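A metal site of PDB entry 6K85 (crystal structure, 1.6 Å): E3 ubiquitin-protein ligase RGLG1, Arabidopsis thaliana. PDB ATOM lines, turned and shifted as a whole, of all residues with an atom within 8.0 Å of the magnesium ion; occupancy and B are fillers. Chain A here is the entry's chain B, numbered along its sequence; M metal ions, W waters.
The magnesium ion is bound by water W2, at 2.0 Å. The magnesium ion is bound by OG of Ser 48, at 2.0 Å. The magnesium ion is bound by OD1 of Asp 168 (2.1 Å). The magnesium ion is bound by water W1 (2.1 Å). Water W3 is bound to the magnesium ion (2.1 Å). OG1 of Thr 46 is bound to the magnesium ion. The magnesium ion has six donor atoms within binding distance.
The backbone carbonyl oxygen (O) of Thr 46 sits at hydrogen-bond distance from the side-chain amide nitrogen (ND2) of Asn 49. The backbone carbonyl oxygen (O) of Asp 44 sits at hydrogen-bond distance from the side-chain hydroxyl (OH) of Tyr 72. The backbone carbonyl oxygen (O) of Ser 48 sits at hydrogen-bond distance from the side-chain hydroxyl (OG1) of Thr 52, at 3.2 Å. The side-chain carboxylate of Asp 168 lies within hydrogen-bond range of the side-chain hydroxyl of Thr 52, 2.8 Å away. The backbone NH of Asp 168 lies within hydrogen-bond range of the side-chain carboxylate of Asp 44 (3.2 Å). The side-chain carboxylate (OD1) of Asp 44 is in hydrogen-bond range of the side-chain amide nitrogen (ND2) of Asn 49, 3.1 Å away. N of Thr 46 is in hydrogen-bond range of OD1 of Asp 44 (2.8 Å). The side-chain carboxylate (OD2) of Asp 168 sits at hydrogen-bond distance from the backbone NH (N) of Asn 49 (3.1 Å).
Residues that only touch the magnesium ion: Asp 44. Within 4 Å of the magnesium ion: Asp 44, Thr 46, Ser 48 and Asp 168. The nearest printed residue that does not touch the magnesium ion is Thr 140 (4.003 Å).
Water W1 lies within hydrogen-bond range of OD2 of Asp 44 and OG1 of Thr 140.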
ATOM      1  N   ASP A  44     -19.592 -16.957  13.274  1.00  0.00           N
ATOM      2  CA  ASP A  44     -20.642 -15.940  13.395  1.00  0.00           C
ATOM      3  C   ASP A  44     -22.012 -16.606  13.334  1.00  0.00           C
ATOM      4  O   ASP A  44     -22.333 -17.274  12.337  1.00  0.00           O
ATOM      5  CB  ASP A  44     -20.453 -14.938  12.249  1.00  0.00           C
ATOM      6  CG  ASP A  44     -21.498 -13.832  12.193  1.00  0.00           C
ATOM      7  OD1 ASP A  44     -22.699 -14.054  12.464  1.00  0.00           O
ATOM      8  OD2 ASP A  44     -21.097 -12.718  11.818  1.00  0.00           O
ATOM      9  N   PHE A  45     -22.806 -16.435  14.393  1.00  0.00           N
ATOM     10  CA  PHE A  45     -24.141 -17.010  14.448  1.00  0.00           C
ATOM     11  C   PHE A  45     -25.187 -15.915  14.607  1.00  0.00           C
ATOM     12  O   PHE A  45     -26.181 -16.065  15.321  1.00  0.00           O
ATOM     13  CB  PHE A  45     -24.245 -18.031  15.599  1.00  0.00           C
ATOM     14  CG  PHE A  45     -23.524 -19.318  15.333  1.00  0.00           C
ATOM     15  CD1 PHE A  45     -23.913 -20.135  14.266  1.00  0.00           C
ATOM     16  CD2 PHE A  45     -22.468 -19.731  16.132  1.00  0.00           C
ATOM     17  CE1 PHE A  45     -23.262 -21.331  14.020  1.00  0.00           C
ATOM     18  CE2 PHE A  45     -21.810 -20.933  15.887  1.00  0.00           C
ATOM     19  CZ  PHE A  45     -22.204 -21.739  14.827  1.00  0.00           C
ATOM     20  N   THR A  46     -24.958 -14.794  13.925  1.00  0.00           N
ATOM     21  CA  THR A  46     -25.898 -13.671  13.967  1.00  0.00           C
ATOM     22  C   THR A  46     -27.123 -13.945  13.092  1.00  0.00           C
ATOM     23  O   THR A  46     -27.056 -14.695  12.110  1.00  0.00           O
ATOM     24  CB  THR A  46     -25.232 -12.358  13.546  1.00  0.00           C
ATOM     25  OG1 THR A  46     -24.678 -12.509  12.222  1.00  0.00           O
ATOM     26  CG2 THR A  46     -24.114 -11.980  14.545  1.00  0.00           C
ATOM     27  N   LYS A  47     -28.237 -13.320  13.472  1.00  0.00           N
ATOM     28  CA  LYS A  47     -29.506 -13.518  12.763  1.00  0.00           C
ATOM     29  C   LYS A  47     -29.455 -13.017  11.320  1.00  0.00           C
ATOM     30  O   LYS A  47     -30.221 -13.492  10.481  1.00  0.00           O
ATOM     31  CB  LYS A  47     -30.643 -12.834  13.520  1.00  0.00           C
ATOM     32  CG  LYS A  47     -32.047 -13.314  13.128  1.00  0.00           C
ATOM     33  CD  LYS A  47     -33.065 -12.591  14.000  1.00  0.00           C
ATOM     34  CE  LYS A  47     -34.415 -13.296  13.967  1.00  0.00           C
ATOM     35  NZ  LYS A  47     -34.963 -13.318  12.606  1.00  0.00           N
ATOM     36  N   SER A  48     -28.564 -12.091  11.023  1.00  0.00           N
ATOM     37  CA  SER A  48     -28.377 -11.600   9.658  1.00  0.00           C
ATOM     38  C   SER A  48     -28.064 -12.710   8.641  1.00  0.00           C
ATOM     39  O   SER A  48     -28.324 -12.566   7.428  1.00  0.00           O
ATOM     40  CB  SER A  48     -27.253 -10.572   9.617  1.00  0.00           C
ATOM     41  OG  SER A  48     -26.018 -11.222   9.843  1.00  0.00           O
ATOM     42  N   ASN A  49     -27.535 -13.825   9.126  1.00  0.00           N
ATOM     43  CA  ASN A  49     -27.184 -14.952   8.265  1.00  0.00           C
ATOM     44  C   ASN A  49     -28.410 -15.434   7.490  1.00  0.00           C
ATOM     45  O   ASN A  49     -28.293 -15.962   6.381  1.00  0.00           O
ATOM     46  CB  ASN A  49     -26.584 -16.087   9.089  1.00  0.00           C
ATOM     47  CG  ASN A  49     -25.106 -15.854   9.381  1.00  0.00           C
ATOM     48  OD1 ASN A  49     -24.265 -16.010   8.504  1.00  0.00           O
ATOM     49  ND2 ASN A  49     -24.781 -15.491  10.621  1.00  0.00           N
ATOM     50  N   GLU A  50     -29.566 -15.195   8.068  1.00  0.00           N
ATOM     51  CA  GLU A  50     -30.816 -15.579   7.414  1.00  0.00           C
ATOM     52  C   GLU A  50     -31.004 -14.904   6.052  1.00  0.00           C
ATOM     53  O   GLU A  50     -31.523 -15.528   5.114  1.00  0.00           O
ATOM     54  CB  GLU A  50     -31.993 -15.263   8.357  1.00  0.00           C
ATOM     55  CG  GLU A  50     -32.038 -16.219   9.545  1.00  0.00           C
ATOM     56  CD  GLU A  50     -33.171 -15.925  10.521  1.00  0.00           C
ATOM     57  OE1 GLU A  50     -33.244 -16.615  11.560  1.00  0.00           O
ATOM     58  OE2 GLU A  50     -33.982 -15.010  10.273  1.00  0.00           O
ATOM     59  N   TRP A  51     -30.550 -13.659   5.922  1.00  0.00           N
ATOM     60  CA  TRP A  51     -30.816 -12.904   4.700  1.00  0.00           C
ATOM     61  C   TRP A  51     -29.596 -12.395   3.908  1.00  0.00           C
ATOM     62  O   TRP A  51     -29.755 -11.781   2.854  1.00  0.00           O
ATOM     63  CB  TRP A  51     -31.726 -11.712   5.020  1.00  0.00           C
ATOM     64  CG  TRP A  51     -31.460 -11.036   6.327  1.00  0.00           C
ATOM     65  CD1 TRP A  51     -32.020 -11.338   7.546  1.00  0.00           C
ATOM     66  CD2 TRP A  51     -30.596  -9.923   6.564  1.00  0.00           C
ATOM     67  NE1 TRP A  51     -31.548 -10.490   8.514  1.00  0.00           N
ATOM     68  CE2 TRP A  51     -30.673  -9.615   7.936  1.00  0.00           C
ATOM     69  CE3 TRP A  51     -29.741  -9.169   5.747  1.00  0.00           C
ATOM     70  CZ2 TRP A  51     -29.936  -8.571   8.506  1.00  0.00           C
ATOM     71  CZ3 TRP A  51     -29.020  -8.129   6.314  1.00  0.00           C
ATOM     72  CH2 TRP A  51     -29.114  -7.844   7.682  1.00  0.00           C
ATOM     73  N   THR A  52     -28.390 -12.655   4.401  1.00  0.00           N
ATOM     74  CA  THR A  52     -27.186 -12.244   3.661  1.00  0.00           C
ATOM     75  C   THR A  52     -26.777 -13.264   2.604  1.00  0.00           C
ATOM     76  O   THR A  52     -25.732 -13.123   1.962  1.00  0.00           O
ATOM     77  CB  THR A  52     -26.002 -12.018   4.604  1.00  0.00           C
ATOM     78  OG1 THR A  52     -25.859 -13.177   5.441  1.00  0.00           O
ATOM     79  CG2 THR A  52     -26.239 -10.806   5.470  1.00  0.00           C
ATOM     80  N   LEU A  62     -27.283 -18.566   5.354  1.00  0.00           N
ATOM     81  CA  LEU A  62     -25.879 -18.913   5.214  1.00  0.00           C
ATOM     82  C   LEU A  62     -25.573 -20.135   6.077  1.00  0.00           C
ATOM     83  O   LEU A  62     -24.601 -20.850   5.852  1.00  0.00           O
ATOM     84  CB  LEU A  62     -24.977 -17.717   5.595  1.00  0.00           C
ATOM     85  CG  LEU A  62     -24.960 -16.525   4.643  1.00  0.00           C
ATOM     86  CD1 LEU A  62     -23.851 -15.553   5.033  1.00  0.00           C
ATOM     87  CD2 LEU A  62     -24.783 -16.976   3.184  1.00  0.00           C
ATOM     88  N   TYR A  72     -19.981 -21.472   5.324  1.00  0.00           N
ATOM     89  CA  TYR A  72     -19.216 -21.728   6.540  1.00  0.00           C
ATOM     90  C   TYR A  72     -18.503 -23.078   6.424  1.00  0.00           C
ATOM     91  O   TYR A  72     -17.317 -23.170   6.701  1.00  0.00           O
ATOM     92  CB  TYR A  72     -20.128 -21.678   7.776  1.00  0.00           C
ATOM     93  CG  TYR A  72     -20.559 -20.277   8.136  1.00  0.00           C
ATOM     94  CD1 TYR A  72     -19.767 -19.468   8.948  1.00  0.00           C
ATOM     95  CD2 TYR A  72     -21.748 -19.744   7.645  1.00  0.00           C
ATOM     96  CE1 TYR A  72     -20.154 -18.162   9.276  1.00  0.00           C
ATOM     97  CE2 TYR A  72     -22.147 -18.454   7.962  1.00  0.00           C
ATOM     98  CZ  TYR A  72     -21.351 -17.674   8.765  1.00  0.00           C
ATOM     99  OH  TYR A  72     -21.753 -16.392   9.051  1.00  0.00           O
ATOM    100  N   PHE A  97     -20.190 -17.169  18.231  1.00  0.00           N
ATOM    101  CA  PHE A  97     -20.507 -15.861  18.800  1.00  0.00           C
ATOM    102  C   PHE A  97     -21.658 -15.240  18.022  1.00  0.00           C
ATOM    103  O   PHE A  97     -21.843 -15.560  16.852  1.00  0.00           O
ATOM    104  CB  PHE A  97     -19.279 -14.941  18.786  1.00  0.00           C
ATOM    105  CG  PHE A  97     -18.746 -14.626  17.398  1.00  0.00           C
ATOM    106  CD1 PHE A  97     -17.808 -15.458  16.804  1.00  0.00           C
ATOM    107  CD2 PHE A  97     -19.197 -13.512  16.702  1.00  0.00           C
ATOM    108  CE1 PHE A  97     -17.318 -15.189  15.520  1.00  0.00           C
ATOM    109  CE2 PHE A  97     -18.720 -13.226  15.426  1.00  0.00           C
ATOM    110  CZ  PHE A  97     -17.774 -14.064  14.832  1.00  0.00           C
ATOM    111  N   GLY A  98     -22.428 -14.363  18.662  1.00  0.00           N
ATOM    112  CA  GLY A  98     -23.490 -13.664  17.964  1.00  0.00           C
ATOM    113  C   GLY A  98     -24.840 -14.339  18.035  1.00  0.00           C
ATOM    114  O   GLY A  98     -25.820 -13.816  17.497  1.00  0.00           O
ATOM    115  N   ALA A 137     -28.645 -14.205  16.769  1.00  0.00           N
ATOM    116  CA  ALA A 137     -28.895 -12.888  17.357  1.00  0.00           C
ATOM    117  C   ALA A 137     -27.937 -11.796  16.851  1.00  0.00           C
ATOM    118  O   ALA A 137     -27.787 -11.572  15.646  1.00  0.00           O
ATOM    119  CB  ALA A 137     -28.842 -12.976  18.881  1.00  0.00           C
ATOM    120  N   GLY A 138     -27.308 -11.091  17.785  1.00  0.00           N
ATOM    121  CA  GLY A 138     -26.334 -10.059  17.456  1.00  0.00           C
ATOM    122  C   GLY A 138     -26.053  -9.188  18.677  1.00  0.00           C
ATOM    123  O   GLY A 138     -26.403  -9.571  19.805  1.00  0.00           O
ATOM    124  N   PRO A 139     -25.397  -8.032  18.476  1.00  0.00           N
ATOM    125  CA  PRO A 139     -24.866  -7.504  17.218  1.00  0.00           C
ATOM    126  C   PRO A 139     -23.480  -8.074  16.937  1.00  0.00           C
ATOM    127  O   PRO A 139     -23.171  -9.124  17.487  1.00  0.00           O
ATOM    128  CB  PRO A 139     -24.818  -5.993  17.469  1.00  0.00           C
ATOM    129  CG  PRO A 139     -24.536  -5.880  18.936  1.00  0.00           C
ATOM    130  CD  PRO A 139     -25.122  -7.111  19.608  1.00  0.00           C
ATOM    131  N   THR A 140     -22.642  -7.404  16.152  1.00  0.00           N
ATOM    132  CA  THR A 140     -21.374  -7.996  15.721  1.00  0.00           C
ATOM    133  C   THR A 140     -20.147  -7.315  16.315  1.00  0.00           C
ATOM    134  O   THR A 140     -19.880  -6.131  16.070  1.00  0.00           O
ATOM    135  CB  THR A 140     -21.265  -7.979  14.178  1.00  0.00           C
ATOM    136  OG1 THR A 140     -22.438  -8.598  13.649  1.00  0.00           O
ATOM    137  CG2 THR A 140     -20.036  -8.745  13.694  1.00  0.00           C
ATOM    138  N   PHE A 142     -15.913  -8.598  17.254  1.00  0.00           N
ATOM    139  CA  PHE A 142     -14.931  -9.671  17.167  1.00  0.00           C
ATOM    140  C   PHE A 142     -14.008  -9.598  18.384  1.00  0.00           C
ATOM    141  O   PHE A 142     -13.060 -10.359  18.489  1.00  0.00           O
ATOM    142  CB  PHE A 142     -14.128  -9.588  15.855  1.00  0.00           C
ATOM    143  CG  PHE A 142     -14.993  -9.619  14.615  1.00  0.00           C
ATOM    144  CD1 PHE A 142     -16.017 -10.533  14.489  1.00  0.00           C
ATOM    145  CD2 PHE A 142     -14.770  -8.711  13.586  1.00  0.00           C
ATOM    146  CE1 PHE A 142     -16.832 -10.553  13.359  1.00  0.00           C
ATOM    147  CE2 PHE A 142     -15.567  -8.725  12.446  1.00  0.00           C
ATOM    148  CZ  PHE A 142     -16.601  -9.651  12.331  1.00  0.00           C
ATOM    149  N   ALA A 167     -17.413 -14.736   9.256  1.00  0.00           N
ATOM    150  CA  ALA A 167     -18.478 -13.825   9.667  1.00  0.00           C
ATOM    151  C   ALA A 167     -19.255 -13.333   8.474  1.00  0.00           C
ATOM    152  O   ALA A 167     -18.726 -13.327   7.370  1.00  0.00           O
ATOM    153  CB  ALA A 167     -17.903 -12.625  10.436  1.00  0.00           C
ATOM    154  N   ASP A 168     -20.506 -12.909   8.682  1.00  0.00           N
ATOM    155  CA  ASP A 168     -21.329 -12.437   7.566  1.00  0.00           C
ATOM    156  C   ASP A 168     -21.551 -10.923   7.610  1.00  0.00           C
ATOM    157  O   ASP A 168     -22.445 -10.398   6.942  1.00  0.00           O
ATOM    158  CB  ASP A 168     -22.680 -13.175   7.529  1.00  0.00           C
ATOM    159  CG  ASP A 168     -23.731 -12.544   8.445  1.00  0.00           C
ATOM    160  OD1 ASP A 168     -23.389 -12.056   9.542  1.00  0.00           O
ATOM    161  OD2 ASP A 168     -24.930 -12.515   8.051  1.00  0.00           O
ATOM    162  N   GLY A 169     -20.742 -10.228   8.399  1.00  0.00           N
ATOM    163  CA  GLY A 169     -20.810  -8.778   8.424  1.00  0.00           C
ATOM    164  C   GLY A 169     -19.624  -8.110   9.090  1.00  0.00           C
ATOM    165  O   GLY A 169     -18.885  -8.747   9.859  1.00  0.00           O
ATOM    166  N   GLN A 170     -19.436  -6.837   8.784  1.00  0.00           N
ATOM    167  CA  GLN A 170     -18.450  -5.989   9.416  1.00  0.00           C
ATOM    168  C   GLN A 170     -18.840  -5.738  10.877  1.00  0.00           C
ATOM    169  O   GLN A 170     -19.992  -5.949  11.258  1.00  0.00           O
ATOM    170  CB  GLN A 170     -18.318  -4.655   8.655  1.00  0.00           C
ATOM    171  CG  GLN A 170     -18.052  -4.811   7.133  1.00  0.00           C
ATOM    172  CD  GLN A 170     -18.043  -3.475   6.367  1.00  0.00           C
ATOM    173  OE1 GLN A 170     -17.628  -3.396   5.188  1.00  0.00           O
ATOM    174  NE2 GLN A 170     -18.498  -2.407   7.033  1.00  0.00           N
ATOM    175  N   THR A 172     -20.234  -4.012  13.991  1.00  0.00           N
ATOM    176  CA  THR A 172     -21.340  -3.053  14.119  1.00  0.00           C
ATOM    177  C   THR A 172     -20.806  -1.634  14.307  1.00  0.00           C
ATOM    178  O   THR A 172     -19.913  -1.408  15.125  1.00  0.00           O
ATOM    179  CB  THR A 172     -22.249  -3.423  15.312  1.00  0.00           C
ATOM    180  OG1 THR A 172     -22.897  -4.669  15.038  1.00  0.00           O
ATOM    181  CG2 THR A 172     -23.316  -2.349  15.552  1.00  0.00           C
ATOM    182  N   GLY A 211     -22.503  -9.386   2.347  1.00  0.00           N
ATOM    183  CA  GLY A 211     -21.906  -8.238   2.992  1.00  0.00           C
ATOM    184  C   GLY A 211     -22.901  -7.129   3.283  1.00  0.00           C
ATOM    185  O   GLY A 211     -23.966  -7.389   3.844  1.00  0.00           O
ATOM    186  N   TRP A 213     -19.044  -5.676   1.966  1.00  0.00           N
ATOM    187  CA  TRP A 213     -17.685  -5.847   2.470  1.00  0.00           C
ATOM    188  C   TRP A 213     -16.776  -4.736   1.959  1.00  0.00           C
ATOM    189  O   TRP A 213     -15.553  -4.812   2.078  1.00  0.00           O
ATOM    190  CB  TRP A 213     -17.141  -7.203   2.054  1.00  0.00           C
ATOM    191  CG  TRP A 213     -17.850  -8.349   2.709  1.00  0.00           C
ATOM    192  CD1 TRP A 213     -18.704  -9.251   2.121  1.00  0.00           C
ATOM    193  CD2 TRP A 213     -17.781  -8.713   4.099  1.00  0.00           C
ATOM    194  NE1 TRP A 213     -19.151 -10.151   3.058  1.00  0.00           N
ATOM    195  CE2 TRP A 213     -18.606  -9.847   4.276  1.00  0.00           C
ATOM    196  CE3 TRP A 213     -17.104  -8.195   5.202  1.00  0.00           C
ATOM    197  CZ2 TRP A 213     -18.775 -10.459   5.524  1.00  0.00           C
ATOM    198  CZ3 TRP A 213     -17.259  -8.807   6.445  1.00  0.00           C
ATOM    199  CH2 TRP A 213     -18.091  -9.937   6.585  1.00  0.00           C
HETATM  200 MG    MG M   1     -24.312 -10.792  10.875  1.00  0.00          MG
HETATM  201  O   HOH W   1     -22.436 -10.439  11.695  1.00  0.00           O
HETATM  202  O   HOH W   2     -25.287  -9.571  12.130  1.00  0.00           O
HETATM  203  O   HOH W   3     -23.959  -9.039   9.695  1.00  0.00           O
